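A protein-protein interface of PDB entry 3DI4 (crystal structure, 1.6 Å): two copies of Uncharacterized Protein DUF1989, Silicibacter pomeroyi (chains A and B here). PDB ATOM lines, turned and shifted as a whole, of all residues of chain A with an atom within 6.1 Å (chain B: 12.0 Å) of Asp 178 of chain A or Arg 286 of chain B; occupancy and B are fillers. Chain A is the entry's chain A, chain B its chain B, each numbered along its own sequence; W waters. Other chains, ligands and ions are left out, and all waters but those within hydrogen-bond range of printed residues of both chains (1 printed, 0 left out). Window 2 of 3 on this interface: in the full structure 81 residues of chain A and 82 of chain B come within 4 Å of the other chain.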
ATOM      1  N   HIS A 165      13.078 -27.800 -17.697  1.00  0.00           N
ATOM      2  CA  HIS A 165      14.039 -26.828 -17.189  1.00  0.00           C
ATOM      3  C   HIS A 165      13.485 -25.697 -16.322  1.00  0.00           C
ATOM      4  O   HIS A 165      14.272 -24.838 -15.876  1.00  0.00           O
ATOM      5  CB  HIS A 165      14.814 -26.224 -18.354  1.00  0.00           C
ATOM      6  CG  HIS A 165      15.466 -27.246 -19.221  1.00  0.00           C
ATOM      7  ND1 HIS A 165      16.214 -28.296 -18.713  1.00  0.00           N
ATOM      8  CD2 HIS A 165      15.477 -27.390 -20.573  1.00  0.00           C
ATOM      9  CE1 HIS A 165      16.696 -29.004 -19.727  1.00  0.00           C
ATOM     10  NE2 HIS A 165      16.253 -28.484 -20.860  1.00  0.00           N
ATOM     11  N   THR A 173      18.346 -21.951  -9.350  1.00  0.00           N
ATOM     12  CA  THR A 173      19.737 -22.108  -9.742  1.00  0.00           C
ATOM     13  C   THR A 173      20.153 -21.001 -10.729  1.00  0.00           C
ATOM     14  O   THR A 173      21.165 -20.331 -10.511  1.00  0.00           O
ATOM     15  CB  THR A 173      19.981 -23.522 -10.347  1.00  0.00           C
ATOM     16  OG1 THR A 173      19.836 -24.469  -9.328  1.00  0.00           O
ATOM     17  CG2 THR A 173      21.408 -23.638 -10.957  1.00  0.00           C
ATOM     18  N   ARG A 174      19.377 -20.809 -11.790  1.00  0.00           N
ATOM     19  CA  ARG A 174      19.684 -19.724 -12.748  1.00  0.00           C
ATOM     20  C   ARG A 174      19.638 -18.353 -12.113  1.00  0.00           C
ATOM     21  O   ARG A 174      20.458 -17.491 -12.423  1.00  0.00           O
ATOM     22  CB  ARG A 174      18.690 -19.716 -13.885  1.00  0.00           C
ATOM     23  CG  ARG A 174      18.717 -20.942 -14.801  1.00  0.00           C
ATOM     24  CD  ARG A 174      17.861 -20.675 -16.077  1.00  0.00           C
ATOM     25  NE  ARG A 174      16.496 -20.272 -15.785  1.00  0.00           N
ATOM     26  CZ  ARG A 174      15.487 -21.093 -15.488  1.00  0.00           C
ATOM     27  NH1 ARG A 174      15.640 -22.413 -15.510  1.00  0.00           N
ATOM     28  NH2 ARG A 174      14.296 -20.591 -15.215  1.00  0.00           N
ATOM     29  N   ALA A 175      18.628 -18.113 -11.278  1.00  0.00           N
ATOM     30  CA  ALA A 175      18.508 -16.806 -10.637  1.00  0.00           C
ATOM     31  C   ALA A 175      19.736 -16.492  -9.769  1.00  0.00           C
ATOM     32  O   ALA A 175      20.232 -15.351  -9.795  1.00  0.00           O
ATOM     33  CB  ALA A 175      17.191 -16.663  -9.851  1.00  0.00           C
ATOM     34  N   LEU A 176      20.181 -17.455  -8.983  1.00  0.00           N
ATOM     35  CA  LEU A 176      21.329 -17.289  -8.077  1.00  0.00           C
ATOM     36  C   LEU A 176      22.604 -17.066  -8.874  1.00  0.00           C
ATOM     37  O   LEU A 176      23.402 -16.196  -8.559  1.00  0.00           O
ATOM     38  CB  LEU A 176      21.513 -18.507  -7.162  1.00  0.00           C
ATOM     39  CG  LEU A 176      22.562 -18.361  -6.060  1.00  0.00           C
ATOM     40  CD1 LEU A 176      22.266 -17.114  -5.136  1.00  0.00           C
ATOM     41  CD2 LEU A 176      22.651 -19.606  -5.238  1.00  0.00           C
ATOM     42  N   ALA A 177      22.796 -17.891  -9.894  1.00  0.00           N
ATOM     43  CA  ALA A 177      23.958 -17.754 -10.782  1.00  0.00           C
ATOM     44  C   ALA A 177      24.000 -16.387 -11.454  1.00  0.00           C
ATOM     45  O   ALA A 177      25.029 -15.691 -11.428  1.00  0.00           O
ATOM     46  CB  ALA A 177      23.922 -18.897 -11.832  1.00  0.00           C
ATOM     47  N   ASP A 178      22.874 -15.973 -12.018  1.00  0.00           N
ATOM     48  CA  ASP A 178      22.776 -14.706 -12.722  1.00  0.00           C
ATOM     49  C   ASP A 178      23.003 -13.529 -11.781  1.00  0.00           C
ATOM     50  O   ASP A 178      23.656 -12.559 -12.171  1.00  0.00           O
ATOM     51  CB  ASP A 178      21.427 -14.536 -13.374  1.00  0.00           C
ATOM     52  CG  ASP A 178      21.184 -15.489 -14.539  1.00  0.00           C
ATOM     53  OD1 ASP A 178      22.106 -16.210 -14.966  1.00  0.00           O
ATOM     54  OD2 ASP A 178      20.019 -15.531 -14.983  1.00  0.00           O
ATOM     55  N   HIS A 179      22.471 -13.583 -10.558  1.00  0.00           N
ATOM     56  CA  HIS A 179      22.671 -12.484  -9.600  1.00  0.00           C
ATOM     57  C   HIS A 179      24.084 -12.379  -9.104  1.00  0.00           C
ATOM     58  O   HIS A 179      24.603 -11.263  -8.930  1.00  0.00           O
ATOM     59  CB  HIS A 179      21.782 -12.644  -8.360  1.00  0.00           C
ATOM     60  CG  HIS A 179      21.647 -11.388  -7.551  1.00  0.00           C
ATOM     61  ND1 HIS A 179      20.683 -10.430  -7.812  1.00  0.00           N
ATOM     62  CD2 HIS A 179      22.350 -10.945  -6.484  1.00  0.00           C
ATOM     63  CE1 HIS A 179      20.811  -9.449  -6.931  1.00  0.00           C
ATOM     64  NE2 HIS A 179      21.825  -9.732  -6.131  1.00  0.00           N
ATOM     65  N   THR A 180      24.682 -13.520  -8.786  1.00  0.00           N
ATOM     66  CA  THR A 180      25.985 -13.564  -8.126  1.00  0.00           C
ATOM     67  C   THR A 180      27.179 -13.723  -9.064  1.00  0.00           C
ATOM     68  O   THR A 180      28.316 -13.524  -8.630  1.00  0.00           O
ATOM     69  CB  THR A 180      26.034 -14.699  -7.129  1.00  0.00           C
ATOM     70  OG1 THR A 180      26.001 -15.959  -7.830  1.00  0.00           O
ATOM     71  CG2 THR A 180      24.875 -14.568  -6.156  1.00  0.00           C
ATOM     72  N   GLY A 181      26.921 -14.091 -10.321  1.00  0.00           N
ATOM     73  CA  GLY A 181      27.986 -14.405 -11.256  1.00  0.00           C
ATOM     74  C   GLY A 181      28.680 -15.718 -10.999  1.00  0.00           C
ATOM     75  O   GLY A 181      29.665 -16.030 -11.678  1.00  0.00           O
ATOM     76  N   LEU A 182      28.165 -16.513 -10.054  1.00  0.00           N
ATOM     77  CA  LEU A 182      28.674 -17.843  -9.801  1.00  0.00           C
ATOM     78  C   LEU A 182      28.422 -18.720 -11.024  1.00  0.00           C
ATOM     79  O   LEU A 182      27.398 -18.553 -11.694  1.00  0.00           O
ATOM     80  CB  LEU A 182      27.997 -18.479  -8.582  1.00  0.00           C
ATOM     81  CG  LEU A 182      28.451 -18.086  -7.175  1.00  0.00           C
ATOM     82  CD1 LEU A 182      27.550 -18.748  -6.122  1.00  0.00           C
ATOM     83  CD2 LEU A 182      29.907 -18.490  -6.941  1.00  0.00           C
ATOM     84  N   LEU A 184      26.973 -21.802 -13.020  1.00  0.00           N
ATOM     85  CA  LEU A 184      25.643 -22.381 -12.817  1.00  0.00           C
ATOM     86  C   LEU A 184      25.647 -23.582 -11.867  1.00  0.00           C
ATOM     87  O   LEU A 184      24.794 -23.700 -10.988  1.00  0.00           O
ATOM     88  CB  LEU A 184      25.060 -22.755 -14.183  1.00  0.00           C
ATOM     89  CG  LEU A 184      23.593 -23.133 -14.236  1.00  0.00           C
ATOM     90  CD1 LEU A 184      22.659 -21.930 -13.998  1.00  0.00           C
ATOM     91  CD2 LEU A 184      23.308 -23.788 -15.606  1.00  0.00           C
ATOM     92  N   TYR B 280      19.019 -36.535 -15.723  1.00  0.00           N
ATOM     93  CA  TYR B 280      18.673 -35.184 -16.158  1.00  0.00           C
ATOM     94  C   TYR B 280      19.865 -34.487 -16.793  1.00  0.00           C
ATOM     95  O   TYR B 280      21.004 -34.653 -16.327  1.00  0.00           O
ATOM     96  CB  TYR B 280      18.097 -34.349 -15.008  1.00  0.00           C
ATOM     97  CG  TYR B 280      17.866 -32.898 -15.389  1.00  0.00           C
ATOM     98  CD1 TYR B 280      17.000 -32.536 -16.432  1.00  0.00           C
ATOM     99  CD2 TYR B 280      18.520 -31.880 -14.701  1.00  0.00           C
ATOM    100  CE1 TYR B 280      16.840 -31.196 -16.803  1.00  0.00           C
ATOM    101  CE2 TYR B 280      18.363 -30.549 -15.060  1.00  0.00           C
ATOM    102  CZ  TYR B 280      17.503 -30.203 -16.087  1.00  0.00           C
ATOM    103  OH  TYR B 280      17.369 -28.875 -16.420  1.00  0.00           O
ATOM    104  N   ASP B 281      19.638 -33.731 -17.872  1.00  0.00           N
ATOM    105  CA  ASP B 281      20.780 -33.152 -18.613  1.00  0.00           C
ATOM    106  C   ASP B 281      21.591 -32.032 -17.875  1.00  0.00           C
ATOM    107  O   ASP B 281      22.664 -31.629 -18.351  1.00  0.00           O
ATOM    108  CB  ASP B 281      20.398 -32.757 -20.053  1.00  0.00           C
ATOM    109  CG  ASP B 281      19.500 -31.560 -20.145  1.00  0.00           C
ATOM    110  OD1 ASP B 281      19.571 -30.633 -19.311  1.00  0.00           O
ATOM    111  OD2 ASP B 281      18.724 -31.510 -21.121  1.00  0.00           O
ATOM    112  N   ARG B 282      21.047 -31.543 -16.753  1.00  0.00           N
ATOM    113  CA  ARG B 282      21.703 -30.586 -15.850  1.00  0.00           C
ATOM    114  C   ARG B 282      21.890 -29.212 -16.499  1.00  0.00           C
ATOM    115  O   ARG B 282      22.630 -28.356 -15.991  1.00  0.00           O
ATOM    116  CB  ARG B 282      23.035 -31.137 -15.321  1.00  0.00           C
ATOM    117  CG  ARG B 282      22.896 -32.455 -14.560  1.00  0.00           C
ATOM    118  CD  ARG B 282      24.003 -32.644 -13.520  1.00  0.00           C
ATOM    119  NE  ARG B 282      24.018 -31.542 -12.561  1.00  0.00           N
ATOM    120  CZ  ARG B 282      25.073 -31.158 -11.859  1.00  0.00           C
ATOM    121  NH1 ARG B 282      26.245 -31.757 -12.003  1.00  0.00           N
ATOM    122  NH2 ARG B 282      24.970 -30.155 -11.026  1.00  0.00           N
ATOM    123  N   SER B 283      21.179 -28.966 -17.609  1.00  0.00           N
ATOM    124  CA  SER B 283      21.355 -27.694 -18.334  1.00  0.00           C
ATOM    125  C   SER B 283      20.546 -26.568 -17.701  1.00  0.00           C
ATOM    126  O   SER B 283      20.894 -25.395 -17.814  1.00  0.00           O
ATOM    127  CB  SER B 283      20.967 -27.843 -19.801  1.00  0.00           C
ATOM    128  OG  SER B 283      19.576 -28.000 -19.948  1.00  0.00           O
ATOM    129  N   HIS B 284      19.465 -26.923 -17.008  1.00  0.00           N
ATOM    130  CA  HIS B 284      18.592 -25.897 -16.376  1.00  0.00           C
ATOM    131  C   HIS B 284      18.075 -24.867 -17.375  1.00  0.00           C
ATOM    132  O   HIS B 284      17.685 -23.758 -17.001  1.00  0.00           O
ATOM    133  CB  HIS B 284      19.273 -25.206 -15.164  1.00  0.00           C
ATOM    134  CG  HIS B 284      19.801 -26.165 -14.155  1.00  0.00           C
ATOM    135  ND1 HIS B 284      18.976 -26.972 -13.397  1.00  0.00           N
ATOM    136  CD2 HIS B 284      21.072 -26.485 -13.806  1.00  0.00           C
ATOM    137  CE1 HIS B 284      19.719 -27.746 -12.625  1.00  0.00           C
ATOM    138  NE2 HIS B 284      20.997 -27.467 -12.850  1.00  0.00           N
ATOM    139  N   GLY B 285      17.993 -25.281 -18.636  1.00  0.00           N
ATOM    140  CA  GLY B 285      17.449 -24.441 -19.690  1.00  0.00           C
ATOM    141  C   GLY B 285      18.498 -23.569 -20.357  1.00  0.00           C
ATOM    142  O   GLY B 285      18.178 -22.818 -21.290  1.00  0.00           O
ATOM    143  N   ARG B 286      19.729 -23.643 -19.878  1.00  0.00           N
ATOM    144  CA  ARG B 286      20.838 -22.854 -20.447  1.00  0.00           C
ATOM    145  C   ARG B 286      21.580 -23.656 -21.531  1.00  0.00           C
ATOM    146  O   ARG B 286      21.320 -24.851 -21.801  1.00  0.00           O
ATOM    147  CB  ARG B 286      21.806 -22.427 -19.341  1.00  0.00           C
ATOM    148  CG  ARG B 286      21.220 -21.390 -18.357  1.00  0.00           C
ATOM    149  CD  ARG B 286      21.235 -20.021 -19.002  1.00  0.00           C
ATOM    150  NE  ARG B 286      20.299 -19.068 -18.414  1.00  0.00           N
ATOM    151  CZ  ARG B 286      20.547 -18.286 -17.365  1.00  0.00           C
ATOM    152  NH1 ARG B 286      21.691 -18.362 -16.701  1.00  0.00           N
ATOM    153  NH2 ARG B 286      19.587 -17.443 -16.961  1.00  0.00           N
ATOM    154  OXT ARG B 286      22.469 -23.115 -22.208  1.00  0.00           O
HETATM  155  O   HOH W   1      17.557 -29.631 -22.988  1.00  0.00           O
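His 165 of chain A touches Asp 281 of chain B.
His 284 of chain B touches His 165 of chain A.
His 165 of chain A touches Gly 285 of chain B (CG to N, 3.3 Å).
Arg 174 of chain A touches Arg 286 of chain B.
Ser 283 of chain B touches Leu 184 of chain A (O to CD2, 3.6 Å).
CD2 of His 284 of chain B touches CD2 of Leu 184 of chain A, 3.9 Å away.
Printed residues of chain A that touch a printed residue of chain B: His 165, Arg 174, Asp 178 and Leu 184.
Among the printed residues, Asp or Glu carboxylates within 4 Å of a Lys or Arg side-chain nitrogen of the other chain: Asp 178 of chain A with Arg 286 of chain B (2.8 Å).
No position is printed for both chains.
Of the 10 pairs that touch across the chains among the printed residues, none has its exchanged pair printed and touching as well.
The guanidinium group (NH2) of Arg 286 of chain B lies within salt-bridge range of the side-chain carboxylate (OD2) of Asp 178 of chain A (2.8 Å).
NE2 of His 165 of chain A lies close to OG of Ser 283 of chain B, 3.5 Å away.
The backbone carbonyl oxygen (O) of His 284 of chain B sits at hydrogen-bond distance from the guanidinium group (NH1) of Arg 174 of chain A (2.9 Å).
A ring nitrogen (ND1) of His 165 of chain A is in hydrogen-bond range of the side-chain hydroxyl of Tyr 280 of chain B (2.6 Å).
Of chain B, only Arg 286 (2.8 Å) comes within 4 Å of Asp 178 of chain A.
Printed residues of chain A within 4 Å of Arg 286 of chain B: Arg 174 and Asp 178.
Arg 174 of chain A touches just these residues of chain B: His 284 (2.9 Å) and Arg 286 (3.7 Å).
No residue of chain B comes within 4 Å of Ala 177 of chain A.
Thr 180 of chain A touches none of the printed residues of chain B.
No residue of chain B comes within 4 Å of Gly 181 of chain A.
Printed residues of chain A within 4 Å of Gly 285 of chain B: His 165.
Of the printed residues of chain B, Leu 184 of chain A touches Ser 283 (3.6 Å) and His 284 (3.9 Å).
Printed residues of chain A within 4 Å of Ser 283 of chain B: His 165 (3.1 Å) and Leu 184 (3.6 Å).
Of the printed residues of chain B, His 165 of chain A touches Tyr 280, Asp 281, Ser 283, His 284 and Gly 285.
Leu 182 of chain A touches none of the printed residues of chain B.
Thr 173 of chain A touches none of the printed residues of chain B.
The nearest residue of chain A that does not touch Arg 286 of chain B is Leu 184 of chain A (4.2 Å).
The backbone NH (N) of His 284 of chain B sits at hydrogen-bond distance from the side-chain hydroxyl (OH) of Tyr 280 of chain B, at 2.9 Å.
OG of Ser 283 of chain B lies close to N of Gly 285 of chain B.
OD1 of Asp 281 of chain B is in hydrogen-bond range of OG of Ser 283 of chain B, 2.7 Å away.
The backbone carbonyl oxygen of His 165 of chain A is in hydrogen-bond range of the guanidinium group of Arg 174 of chain A (2.8 Å).
Water W1 bridges NE2 of His 165 of chain A and OD2 of Asp 281 of chain B.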
